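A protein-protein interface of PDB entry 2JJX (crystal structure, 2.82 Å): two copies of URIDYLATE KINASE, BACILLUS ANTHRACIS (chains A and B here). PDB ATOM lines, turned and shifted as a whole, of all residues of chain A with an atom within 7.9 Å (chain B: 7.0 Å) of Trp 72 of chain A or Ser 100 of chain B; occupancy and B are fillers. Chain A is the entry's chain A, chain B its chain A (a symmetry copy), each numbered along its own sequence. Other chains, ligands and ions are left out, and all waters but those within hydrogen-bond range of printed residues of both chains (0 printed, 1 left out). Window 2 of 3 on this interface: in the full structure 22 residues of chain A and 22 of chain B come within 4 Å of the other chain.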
ATOM      1  N   PHE A  64      -7.165 -12.286  14.605  1.00  0.00           N
ATOM      2  CA  PHE A  64      -6.717 -10.964  14.196  1.00  0.00           C
ATOM      3  C   PHE A  64      -6.303 -10.071  15.353  1.00  0.00           C
ATOM      4  O   PHE A  64      -7.017  -9.957  16.351  1.00  0.00           O
ATOM      5  CB  PHE A  64      -7.824 -10.272  13.400  1.00  0.00           C
ATOM      6  CG  PHE A  64      -7.372  -9.029  12.694  1.00  0.00           C
ATOM      7  CD1 PHE A  64      -6.391  -9.099  11.728  1.00  0.00           C
ATOM      8  CD2 PHE A  64      -7.826  -7.781  13.096  1.00  0.00           C
ATOM      9  CE1 PHE A  64      -5.921  -7.965  11.132  1.00  0.00           C
ATOM     10  CE2 PHE A  64      -7.369  -6.645  12.482  1.00  0.00           C
ATOM     11  CZ  PHE A  64      -6.413  -6.740  11.505  1.00  0.00           C
ATOM     12  N   GLY A  66      -4.337  -5.987  16.177  1.00  0.00           N
ATOM     13  CA  GLY A  66      -3.923  -4.667  15.731  1.00  0.00           C
ATOM     14  C   GLY A  66      -2.476  -4.608  15.289  1.00  0.00           C
ATOM     15  O   GLY A  66      -2.044  -3.621  14.684  1.00  0.00           O
ATOM     16  N   HIS A  67      -1.732  -5.669  15.578  1.00  0.00           N
ATOM     17  CA  HIS A  67      -0.341  -5.740  15.170  1.00  0.00           C
ATOM     18  C   HIS A  67      -0.189  -5.474  13.671  1.00  0.00           C
ATOM     19  O   HIS A  67       0.774  -4.850  13.236  1.00  0.00           O
ATOM     20  CB  HIS A  67       0.253  -7.096  15.543  1.00  0.00           C
ATOM     21  CG  HIS A  67       0.828  -7.143  16.925  1.00  0.00           C
ATOM     22  ND1 HIS A  67       1.455  -6.062  17.503  1.00  0.00           N
ATOM     23  CD2 HIS A  67       0.908  -8.152  17.828  1.00  0.00           C
ATOM     24  CE1 HIS A  67       1.890  -6.398  18.707  1.00  0.00           C
ATOM     25  NE2 HIS A  67       1.571  -7.658  18.928  1.00  0.00           N
ATOM     26  N   LEU A  68      -1.165  -5.918  12.887  1.00  0.00           N
ATOM     27  CA  LEU A  68      -1.167  -5.718  11.443  1.00  0.00           C
ATOM     28  C   LEU A  68      -1.676  -4.352  11.131  1.00  0.00           C
ATOM     29  O   LEU A  68      -1.006  -3.571  10.482  1.00  0.00           O
ATOM     30  CB  LEU A  68      -2.132  -6.689  10.765  1.00  0.00           C
ATOM     31  CG  LEU A  68      -1.649  -8.128  10.647  1.00  0.00           C
ATOM     32  CD1 LEU A  68      -0.195  -8.114  10.234  1.00  0.00           C
ATOM     33  CD2 LEU A  68      -1.862  -8.866  11.952  1.00  0.00           C
ATOM     34  N   ALA A  69      -2.927  -4.128  11.523  1.00  0.00           N
ATOM     35  CA  ALA A  69      -3.653  -2.872  11.298  1.00  0.00           C
ATOM     36  C   ALA A  69      -2.687  -1.702  11.268  1.00  0.00           C
ATOM     37  O   ALA A  69      -2.694  -0.910  10.325  1.00  0.00           O
ATOM     38  CB  ALA A  69      -4.688  -2.655  12.387  1.00  0.00           C
ATOM     39  N   GLU A  70      -1.809  -1.658  12.267  1.00  0.00           N
ATOM     40  CA  GLU A  70      -0.777  -0.637  12.361  1.00  0.00           C
ATOM     41  C   GLU A  70       0.165  -0.767  11.168  1.00  0.00           C
ATOM     42  O   GLU A  70       0.481   0.219  10.497  1.00  0.00           O
ATOM     43  CB  GLU A  70       0.006  -0.809  13.666  1.00  0.00           C
ATOM     44  CG  GLU A  70       1.067   0.274  13.926  1.00  0.00           C
ATOM     45  CD  GLU A  70       1.764   0.122  15.284  1.00  0.00           C
ATOM     46  OE1 GLU A  70       1.501  -0.892  15.984  1.00  0.00           O
ATOM     47  OE2 GLU A  70       2.573   1.017  15.646  1.00  0.00           O
ATOM     48  N   GLU A  71       0.588  -2.001  10.908  1.00  0.00           N
ATOM     49  CA  GLU A  71       1.535  -2.287   9.843  1.00  0.00           C
ATOM     50  C   GLU A  71       1.084  -1.718   8.513  1.00  0.00           C
ATOM     51  O   GLU A  71       1.899  -1.254   7.713  1.00  0.00           O
ATOM     52  CB  GLU A  71       1.768  -3.787   9.703  1.00  0.00           C
ATOM     53  CG  GLU A  71       2.594  -4.401  10.834  1.00  0.00           C
ATOM     54  CD  GLU A  71       2.774  -5.906  10.684  1.00  0.00           C
ATOM     55  OE1 GLU A  71       2.756  -6.394   9.529  1.00  0.00           O
ATOM     56  OE2 GLU A  71       2.866  -6.602  11.721  1.00  0.00           O
ATOM     57  N   TRP A  72      -0.212  -1.806   8.247  1.00  0.00           N
ATOM     58  CA  TRP A  72      -0.738  -1.315   6.993  1.00  0.00           C
ATOM     59  C   TRP A  72      -1.620  -0.105   7.192  1.00  0.00           C
ATOM     60  O   TRP A  72      -2.341   0.292   6.278  1.00  0.00           O
ATOM     61  CB  TRP A  72      -1.495  -2.426   6.292  1.00  0.00           C
ATOM     62  CG  TRP A  72      -0.723  -3.713   6.247  1.00  0.00           C
ATOM     63  CD1 TRP A  72      -0.726  -4.705   7.197  1.00  0.00           C
ATOM     64  CD2 TRP A  72       0.212  -4.132   5.241  1.00  0.00           C
ATOM     65  NE1 TRP A  72       0.073  -5.751   6.800  1.00  0.00           N
ATOM     66  CE2 TRP A  72       0.662  -5.426   5.602  1.00  0.00           C
ATOM     67  CE3 TRP A  72       0.646  -3.582   4.024  1.00  0.00           C
ATOM     68  CZ2 TRP A  72       1.560  -6.156   4.825  1.00  0.00           C
ATOM     69  CZ3 TRP A  72       1.502  -4.345   3.221  1.00  0.00           C
ATOM     70  CH2 TRP A  72       1.975  -5.599   3.647  1.00  0.00           C
ATOM     71  N   GLY A  73      -1.542   0.478   8.388  1.00  0.00           N
ATOM     72  CA  GLY A  73      -2.279   1.672   8.765  1.00  0.00           C
ATOM     73  C   GLY A  73      -3.764   1.622   8.461  1.00  0.00           C
ATOM     74  O   GLY A  73      -4.310   2.534   7.836  1.00  0.00           O
ATOM     75  N   ILE A  74      -4.427   0.572   8.937  1.00  0.00           N
ATOM     76  CA  ILE A  74      -5.861   0.455   8.742  1.00  0.00           C
ATOM     77  C   ILE A  74      -6.535   1.257   9.834  1.00  0.00           C
ATOM     78  O   ILE A  74      -6.193   1.110  11.003  1.00  0.00           O
ATOM     79  CB  ILE A  74      -6.320  -1.012   8.809  1.00  0.00           C
ATOM     80  CG1 ILE A  74      -5.716  -1.824   7.665  1.00  0.00           C
ATOM     81  CG2 ILE A  74      -7.828  -1.106   8.811  1.00  0.00           C
ATOM     82  CD1 ILE A  74      -6.032  -3.311   7.750  1.00  0.00           C
ATOM     83  N   ASP A  75      -7.503   2.085   9.457  1.00  0.00           N
ATOM     84  CA  ASP A  75      -8.246   2.864  10.443  1.00  0.00           C
ATOM     85  C   ASP A  75      -8.706   2.008  11.613  1.00  0.00           C
ATOM     86  O   ASP A  75      -9.299   0.934  11.438  1.00  0.00           O
ATOM     87  CB  ASP A  75      -9.458   3.565   9.823  1.00  0.00           C
ATOM     88  CG  ASP A  75      -9.953   4.728  10.660  1.00  0.00           C
ATOM     89  OD1 ASP A  75      -9.605   4.808  11.855  1.00  0.00           O
ATOM     90  OD2 ASP A  75     -10.633   5.606  10.098  1.00  0.00           O
ATOM     91  N   PHE B  32      -2.076 -14.434   8.747  1.00  0.00           N
ATOM     92  CA  PHE B  32      -1.558 -13.579   7.699  1.00  0.00           C
ATOM     93  C   PHE B  32      -0.063 -13.462   7.815  1.00  0.00           C
ATOM     94  O   PHE B  32       0.496 -13.537   8.898  1.00  0.00           O
ATOM     95  CB  PHE B  32      -2.176 -12.194   7.771  1.00  0.00           C
ATOM     96  CG  PHE B  32      -3.669 -12.210   7.755  1.00  0.00           C
ATOM     97  CD1 PHE B  32      -4.367 -12.456   8.922  1.00  0.00           C
ATOM     98  CD2 PHE B  32      -4.375 -11.999   6.579  1.00  0.00           C
ATOM     99  CE1 PHE B  32      -5.730 -12.455   8.928  1.00  0.00           C
ATOM    100  CE2 PHE B  32      -5.740 -11.984   6.590  1.00  0.00           C
ATOM    101  CZ  PHE B  32      -6.419 -12.227   7.763  1.00  0.00           C
ATOM    102  N   ASN B  33       0.566 -13.224   6.681  1.00  0.00           N
ATOM    103  CA  ASN B  33       1.993 -13.037   6.592  1.00  0.00           C
ATOM    104  C   ASN B  33       2.148 -11.777   5.758  1.00  0.00           C
ATOM    105  O   ASN B  33       1.713 -11.747   4.600  1.00  0.00           O
ATOM    106  CB  ASN B  33       2.592 -14.231   5.852  1.00  0.00           C
ATOM    107  CG  ASN B  33       4.097 -14.128   5.703  1.00  0.00           C
ATOM    108  OD1 ASN B  33       4.603 -13.552   4.726  1.00  0.00           O
ATOM    109  ND2 ASN B  33       4.825 -14.668   6.685  1.00  0.00           N
ATOM    110  N   SER B  34       2.663 -10.713   6.373  1.00  0.00           N
ATOM    111  CA  SER B  34       2.789  -9.431   5.678  1.00  0.00           C
ATOM    112  C   SER B  34       3.746  -9.452   4.486  1.00  0.00           C
ATOM    113  O   SER B  34       3.688  -8.595   3.598  1.00  0.00           O
ATOM    114  CB  SER B  34       3.141  -8.305   6.646  1.00  0.00           C
ATOM    115  OG  SER B  34       3.907  -8.810   7.725  1.00  0.00           O
ATOM    116  N   LYS B  35       4.586 -10.477   4.427  1.00  0.00           N
ATOM    117  CA  LYS B  35       5.468 -10.606   3.281  1.00  0.00           C
ATOM    118  C   LYS B  35       4.614 -11.107   2.115  1.00  0.00           C
ATOM    119  O   LYS B  35       4.673 -10.575   1.002  1.00  0.00           O
ATOM    120  CB  LYS B  35       6.619 -11.569   3.587  1.00  0.00           C
ATOM    121  CG  LYS B  35       7.821 -10.907   4.249  1.00  0.00           C
ATOM    122  CD  LYS B  35       8.178  -9.576   3.602  1.00  0.00           C
ATOM    123  CE  LYS B  35       7.940  -8.401   4.555  1.00  0.00           C
ATOM    124  NZ  LYS B  35       7.231  -7.242   3.921  1.00  0.00           N
ATOM    125  N   ARG B  36       3.783 -12.109   2.406  1.00  0.00           N
ATOM    126  CA  ARG B  36       2.818 -12.672   1.459  1.00  0.00           C
ATOM    127  C   ARG B  36       1.759 -11.648   1.045  1.00  0.00           C
ATOM    128  O   ARG B  36       1.439 -11.538  -0.140  1.00  0.00           O
ATOM    129  CB  ARG B  36       2.117 -13.881   2.074  1.00  0.00           C
ATOM    130  CG  ARG B  36       3.006 -15.114   2.193  1.00  0.00           C
ATOM    131  CD  ARG B  36       2.250 -16.345   1.736  1.00  0.00           C
ATOM    132  NE  ARG B  36       3.001 -17.588   1.864  1.00  0.00           N
ATOM    133  CZ  ARG B  36       3.195 -18.441   0.862  1.00  0.00           C
ATOM    134  NH1 ARG B  36       2.739 -18.143  -0.351  1.00  0.00           N
ATOM    135  NH2 ARG B  36       3.858 -19.577   1.067  1.00  0.00           N
ATOM    136  N   LEU B  37       1.205 -10.908   2.010  1.00  0.00           N
ATOM    137  CA  LEU B  37       0.223  -9.867   1.701  1.00  0.00           C
ATOM    138  C   LEU B  37       0.814  -8.812   0.760  1.00  0.00           C
ATOM    139  O   LEU B  37       0.113  -8.257  -0.089  1.00  0.00           O
ATOM    140  CB  LEU B  37      -0.277  -9.199   2.980  1.00  0.00           C
ATOM    141  CG  LEU B  37      -1.555  -9.764   3.611  1.00  0.00           C
ATOM    142  CD1 LEU B  37      -1.706 -11.215   3.209  1.00  0.00           C
ATOM    143  CD2 LEU B  37      -1.479  -9.650   5.128  1.00  0.00           C
ATOM    144  N   GLU B  38       2.108  -8.538   0.910  1.00  0.00           N
ATOM    145  CA  GLU B  38       2.796  -7.535   0.091  1.00  0.00           C
ATOM    146  C   GLU B  38       2.967  -8.062  -1.329  1.00  0.00           C
ATOM    147  O   GLU B  38       2.782  -7.324  -2.305  1.00  0.00           O
ATOM    148  CB  GLU B  38       4.169  -7.227   0.682  1.00  0.00           C
ATOM    149  CG  GLU B  38       4.960  -6.193  -0.076  1.00  0.00           C
ATOM    150  CD  GLU B  38       6.362  -6.007   0.487  1.00  0.00           C
ATOM    151  OE1 GLU B  38       6.698  -6.657   1.506  1.00  0.00           O
ATOM    152  OE2 GLU B  38       7.122  -5.194  -0.085  1.00  0.00           O
ATOM    153  N   HIS B  39       3.312  -9.345  -1.440  1.00  0.00           N
ATOM    154  CA  HIS B  39       3.442  -9.982  -2.734  1.00  0.00           C
ATOM    155  C   HIS B  39       2.097  -9.865  -3.459  1.00  0.00           C
ATOM    156  O   HIS B  39       2.025  -9.367  -4.573  1.00  0.00           O
ATOM    157  CB  HIS B  39       3.829 -11.458  -2.567  1.00  0.00           C
ATOM    158  CG  HIS B  39       3.971 -12.180  -3.871  1.00  0.00           C
ATOM    159  ND1 HIS B  39       4.887 -11.788  -4.828  1.00  0.00           N
ATOM    160  CD2 HIS B  39       3.204 -13.125  -4.465  1.00  0.00           C
ATOM    161  CE1 HIS B  39       4.721 -12.507  -5.925  1.00  0.00           C
ATOM    162  NE2 HIS B  39       3.717 -13.338  -5.721  1.00  0.00           N
ATOM    163  N   ALA B  41      -0.428  -7.860  -3.010  1.00  0.00           N
ATOM    164  CA  ALA B  41      -0.790  -6.488  -3.348  1.00  0.00           C
ATOM    165  C   ALA B  41      -0.073  -6.067  -4.626  1.00  0.00           C
ATOM    166  O   ALA B  41      -0.665  -5.468  -5.518  1.00  0.00           O
ATOM    167  CB  ALA B  41      -0.455  -5.555  -2.198  1.00  0.00           C
ATOM    168  N   LEU B  45      -1.572  -4.961  -8.239  1.00  0.00           N
ATOM    169  CA  LEU B  45      -1.402  -3.598  -8.702  1.00  0.00           C
ATOM    170  C   LEU B  45      -0.757  -3.564 -10.070  1.00  0.00           C
ATOM    171  O   LEU B  45      -1.217  -2.850 -10.962  1.00  0.00           O
ATOM    172  CB  LEU B  45      -0.610  -2.785  -7.688  1.00  0.00           C
ATOM    173  CG  LEU B  45      -1.469  -2.679  -6.425  1.00  0.00           C
ATOM    174  CD1 LEU B  45      -0.777  -2.052  -5.191  1.00  0.00           C
ATOM    175  CD2 LEU B  45      -2.763  -1.968  -6.818  1.00  0.00           C
ATOM    176  N   MET B  93      -8.849  -7.278   5.310  1.00  0.00           N
ATOM    177  CA  MET B  93      -7.389  -7.164   5.374  1.00  0.00           C
ATOM    178  C   MET B  93      -6.840  -6.702   4.031  1.00  0.00           C
ATOM    179  O   MET B  93      -6.412  -5.569   3.903  1.00  0.00           O
ATOM    180  CB  MET B  93      -6.738  -8.487   5.733  1.00  0.00           C
ATOM    181  CG  MET B  93      -6.410  -8.605   7.214  1.00  0.00           C
ATOM    182  SD  MET B  93      -5.112  -7.483   7.842  1.00  0.00           S
ATOM    183  CE  MET B  93      -3.867  -7.815   6.691  1.00  0.00           C
ATOM    184  N   LEU B  94      -6.902  -7.566   3.027  1.00  0.00           N
ATOM    185  CA  LEU B  94      -6.498  -7.259   1.653  1.00  0.00           C
ATOM    186  C   LEU B  94      -6.805  -5.818   1.246  1.00  0.00           C
ATOM    187  O   LEU B  94      -5.986  -5.149   0.616  1.00  0.00           O
ATOM    188  CB  LEU B  94      -7.212  -8.213   0.684  1.00  0.00           C
ATOM    189  CG  LEU B  94      -6.534  -8.661  -0.614  1.00  0.00           C
ATOM    190  CD1 LEU B  94      -7.335  -8.221  -1.818  1.00  0.00           C
ATOM    191  CD2 LEU B  94      -5.088  -8.228  -0.740  1.00  0.00           C
ATOM    192  N   ARG B  95      -7.996  -5.340   1.589  1.00  0.00           N
ATOM    193  CA  ARG B  95      -8.351  -3.976   1.244  1.00  0.00           C
ATOM    194  C   ARG B  95      -7.408  -3.001   1.963  1.00  0.00           C
ATOM    195  O   ARG B  95      -6.893  -2.062   1.369  1.00  0.00           O
ATOM    196  CB  ARG B  95      -9.797  -3.697   1.629  1.00  0.00           C
ATOM    197  CG  ARG B  95     -10.358  -2.509   0.908  1.00  0.00           C
ATOM    198  CD  ARG B  95     -10.740  -1.405   1.849  1.00  0.00           C
ATOM    199  NE  ARG B  95     -10.762  -1.842   3.237  1.00  0.00           N
ATOM    200  CZ  ARG B  95     -11.870  -1.919   3.965  1.00  0.00           C
ATOM    201  NH1 ARG B  95     -13.050  -1.635   3.412  1.00  0.00           N
ATOM    202  NH2 ARG B  95     -11.808  -2.312   5.234  1.00  0.00           N
ATOM    203  N   GLY B  96      -7.177  -3.222   3.251  1.00  0.00           N
ATOM    204  CA  GLY B  96      -6.260  -2.391   3.999  1.00  0.00           C
ATOM    205  C   GLY B  96      -4.926  -2.305   3.284  1.00  0.00           C
ATOM    206  O   GLY B  96      -4.427  -1.216   3.006  1.00  0.00           O
ATOM    207  N   VAL B  97      -4.350  -3.472   3.019  1.00  0.00           N
ATOM    208  CA  VAL B  97      -3.079  -3.598   2.332  1.00  0.00           C
ATOM    209  C   VAL B  97      -3.096  -2.834   1.010  1.00  0.00           C
ATOM    210  O   VAL B  97      -2.198  -2.059   0.701  1.00  0.00           O
ATOM    211  CB  VAL B  97      -2.808  -5.085   2.058  1.00  0.00           C
ATOM    212  CG1 VAL B  97      -1.400  -5.287   1.558  1.00  0.00           C
ATOM    213  CG2 VAL B  97      -3.067  -5.911   3.309  1.00  0.00           C
ATOM    214  N   LEU B  98      -4.110  -3.098   0.201  1.00  0.00           N
ATOM    215  CA  LEU B  98      -4.204  -2.465  -1.106  1.00  0.00           C
ATOM    216  C   LEU B  98      -4.274  -0.954  -1.002  1.00  0.00           C
ATOM    217  O   LEU B  98      -3.629  -0.266  -1.776  1.00  0.00           O
ATOM    218  CB  LEU B  98      -5.400  -3.003  -1.902  1.00  0.00           C
ATOM    219  CG  LEU B  98      -5.156  -3.982  -3.059  1.00  0.00           C
ATOM    220  CD1 LEU B  98      -3.850  -4.711  -2.938  1.00  0.00           C
ATOM    221  CD2 LEU B  98      -6.278  -4.999  -3.123  1.00  0.00           C
ATOM    222  N   THR B  99      -5.048  -0.442  -0.051  1.00  0.00           N
ATOM    223  CA  THR B  99      -5.200   0.999   0.154  1.00  0.00           C
ATOM    224  C   THR B  99      -3.868   1.677   0.459  1.00  0.00           C
ATOM    225  O   THR B  99      -3.578   2.773  -0.024  1.00  0.00           O
ATOM    226  CB  THR B  99      -6.196   1.272   1.271  1.00  0.00           C
ATOM    227  OG1 THR B  99      -7.477   0.778   0.881  1.00  0.00           O
ATOM    228  CG2 THR B  99      -6.314   2.768   1.523  1.00  0.00           C
ATOM    229  N   SER B 100      -3.072   1.021   1.295  1.00  0.00           N
ATOM    230  CA  SER B 100      -1.783   1.541   1.693  1.00  0.00           C
ATOM    231  C   SER B 100      -0.857   1.779   0.492  1.00  0.00           C
ATOM    232  O   SER B 100      -0.032   2.695   0.523  1.00  0.00           O
ATOM    233  CB  SER B 100      -1.116   0.599   2.689  1.00  0.00           C
ATOM    234  OG  SER B 100      -0.424  -0.416   1.992  1.00  0.00           O
ATOM    235  N   LYS B 101      -1.008   0.982  -0.565  1.00  0.00           N
ATOM    236  CA  LYS B 101      -0.128   1.064  -1.729  1.00  0.00           C
ATOM    237  C   LYS B 101      -0.690   1.720  -2.971  1.00  0.00           C
ATOM    238  O   LYS B 101       0.046   2.010  -3.911  1.00  0.00           O
ATOM    239  CB  LYS B 101       0.398  -0.321  -2.081  1.00  0.00           C
ATOM    240  CG  LYS B 101       1.385  -0.856  -1.083  1.00  0.00           C
ATOM    241  CD  LYS B 101       1.070  -2.296  -0.780  1.00  0.00           C
ATOM    242  CE  LYS B 101       2.024  -3.227  -1.519  1.00  0.00           C
ATOM    243  NZ  LYS B 101       3.447  -3.129  -1.044  1.00  0.00           N
ATOM    244  N   THR B 102      -2.003   1.874  -3.025  1.00  0.00           N
ATOM    245  CA  THR B 102      -2.628   2.471  -4.201  1.00  0.00           C
ATOM    246  C   THR B 102      -3.366   3.739  -3.825  1.00  0.00           C
ATOM    247  O   THR B 102      -3.588   4.024  -2.652  1.00  0.00           O
ATOM    248  CB  THR B 102      -3.593   1.477  -4.876  1.00  0.00           C
ATOM    249  OG1 THR B 102      -2.864   0.311  -5.272  1.00  0.00           O
ATOM    250  CG2 THR B 102      -4.244   2.091  -6.095  1.00  0.00           C
ATOM    251  N   ASN B 103      -3.775   4.485  -4.835  1.00  0.00           N
ATOM    252  CA  ASN B 103      -4.522   5.708  -4.604  1.00  0.00           C
ATOM    253  C   ASN B 103      -5.909   5.378  -5.102  1.00  0.00           C
ATOM    254  O   ASN B 103      -6.867   6.123  -4.874  1.00  0.00           O
ATOM    255  CB  ASN B 103      -3.951   6.847  -5.445  1.00  0.00           C
ATOM    256  CG  ASN B 103      -3.139   7.806  -4.624  1.00  0.00           C
ATOM    257  OD1 ASN B 103      -3.391   7.967  -3.429  1.00  0.00           O
ATOM    258  ND2 ASN B 103      -2.134   8.420  -5.240  1.00  0.00           N
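The side-chain hydroxyl (OG) of Ser 34 of chain B lies within hydrogen-bond range of the side-chain carboxylate (OE1) of Glu 71 of chain A.
O of Ala 69 of chain A sits at hydrogen-bond distance from N of Ile 74 of chain A, 2.7 Å away.
The backbone carbonyl oxygen (O) of Val 97 of chain B is in hydrogen-bond range of the side-chain hydroxyl (OG) of Ser 100 of chain B.
Phe 64 of chain A touches Met 93 of chain B.
Ser 34 of chain B touches Trp 72 of chain A.
Val 97 of chain B touches Trp 72 of chain A (CG1 to CZ3, 3.5 Å).
CB of Ser 100 of chain B touches O of Trp 72 of chain A, 3.8 Å away.
Ile 74 of chain A touches Gly 96 of chain B.
Printed residues of chain B within 4 Å of Glu 71 of chain A: Ser 34.
Printed residues of chain B within 4 Å of Trp 72 of chain A: Ser 34, Val 97 and Ser 100.
Phe 32 of chain B touches none of the printed residues of chain A.
Of the printed residues of chain A, Ser 34 of chain B touches Glu 71 (3.2 Å) and Trp 72 (3.2 Å).
Leu 94 of chain B touches none of the printed residues of chain A.
Printed residues of chain A within 4 Å of Ser 100 of chain B: Trp 72.
The nearest printed residue of chain B that does not touch Glu 71 of chain A is Ser 100 of chain B (6.1 Å).
Hydrophobic or aromatic side chains of chain B that line the printed part of chain A: Met 93 and Val 97.
Of the 11 printed residues of chain A, 4 touch a printed residue of chain B.
Along chain A the printed residues that touch a printed residue of chain B span positions 64 to 74.
Among the printed residues, 6 pairs touch across the chains.
Among the printed residues, no Asp or Glu carboxylate lies within 4 Å of a Lys or Arg side-chain nitrogen of the other chain.
No position is printed for both chains.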
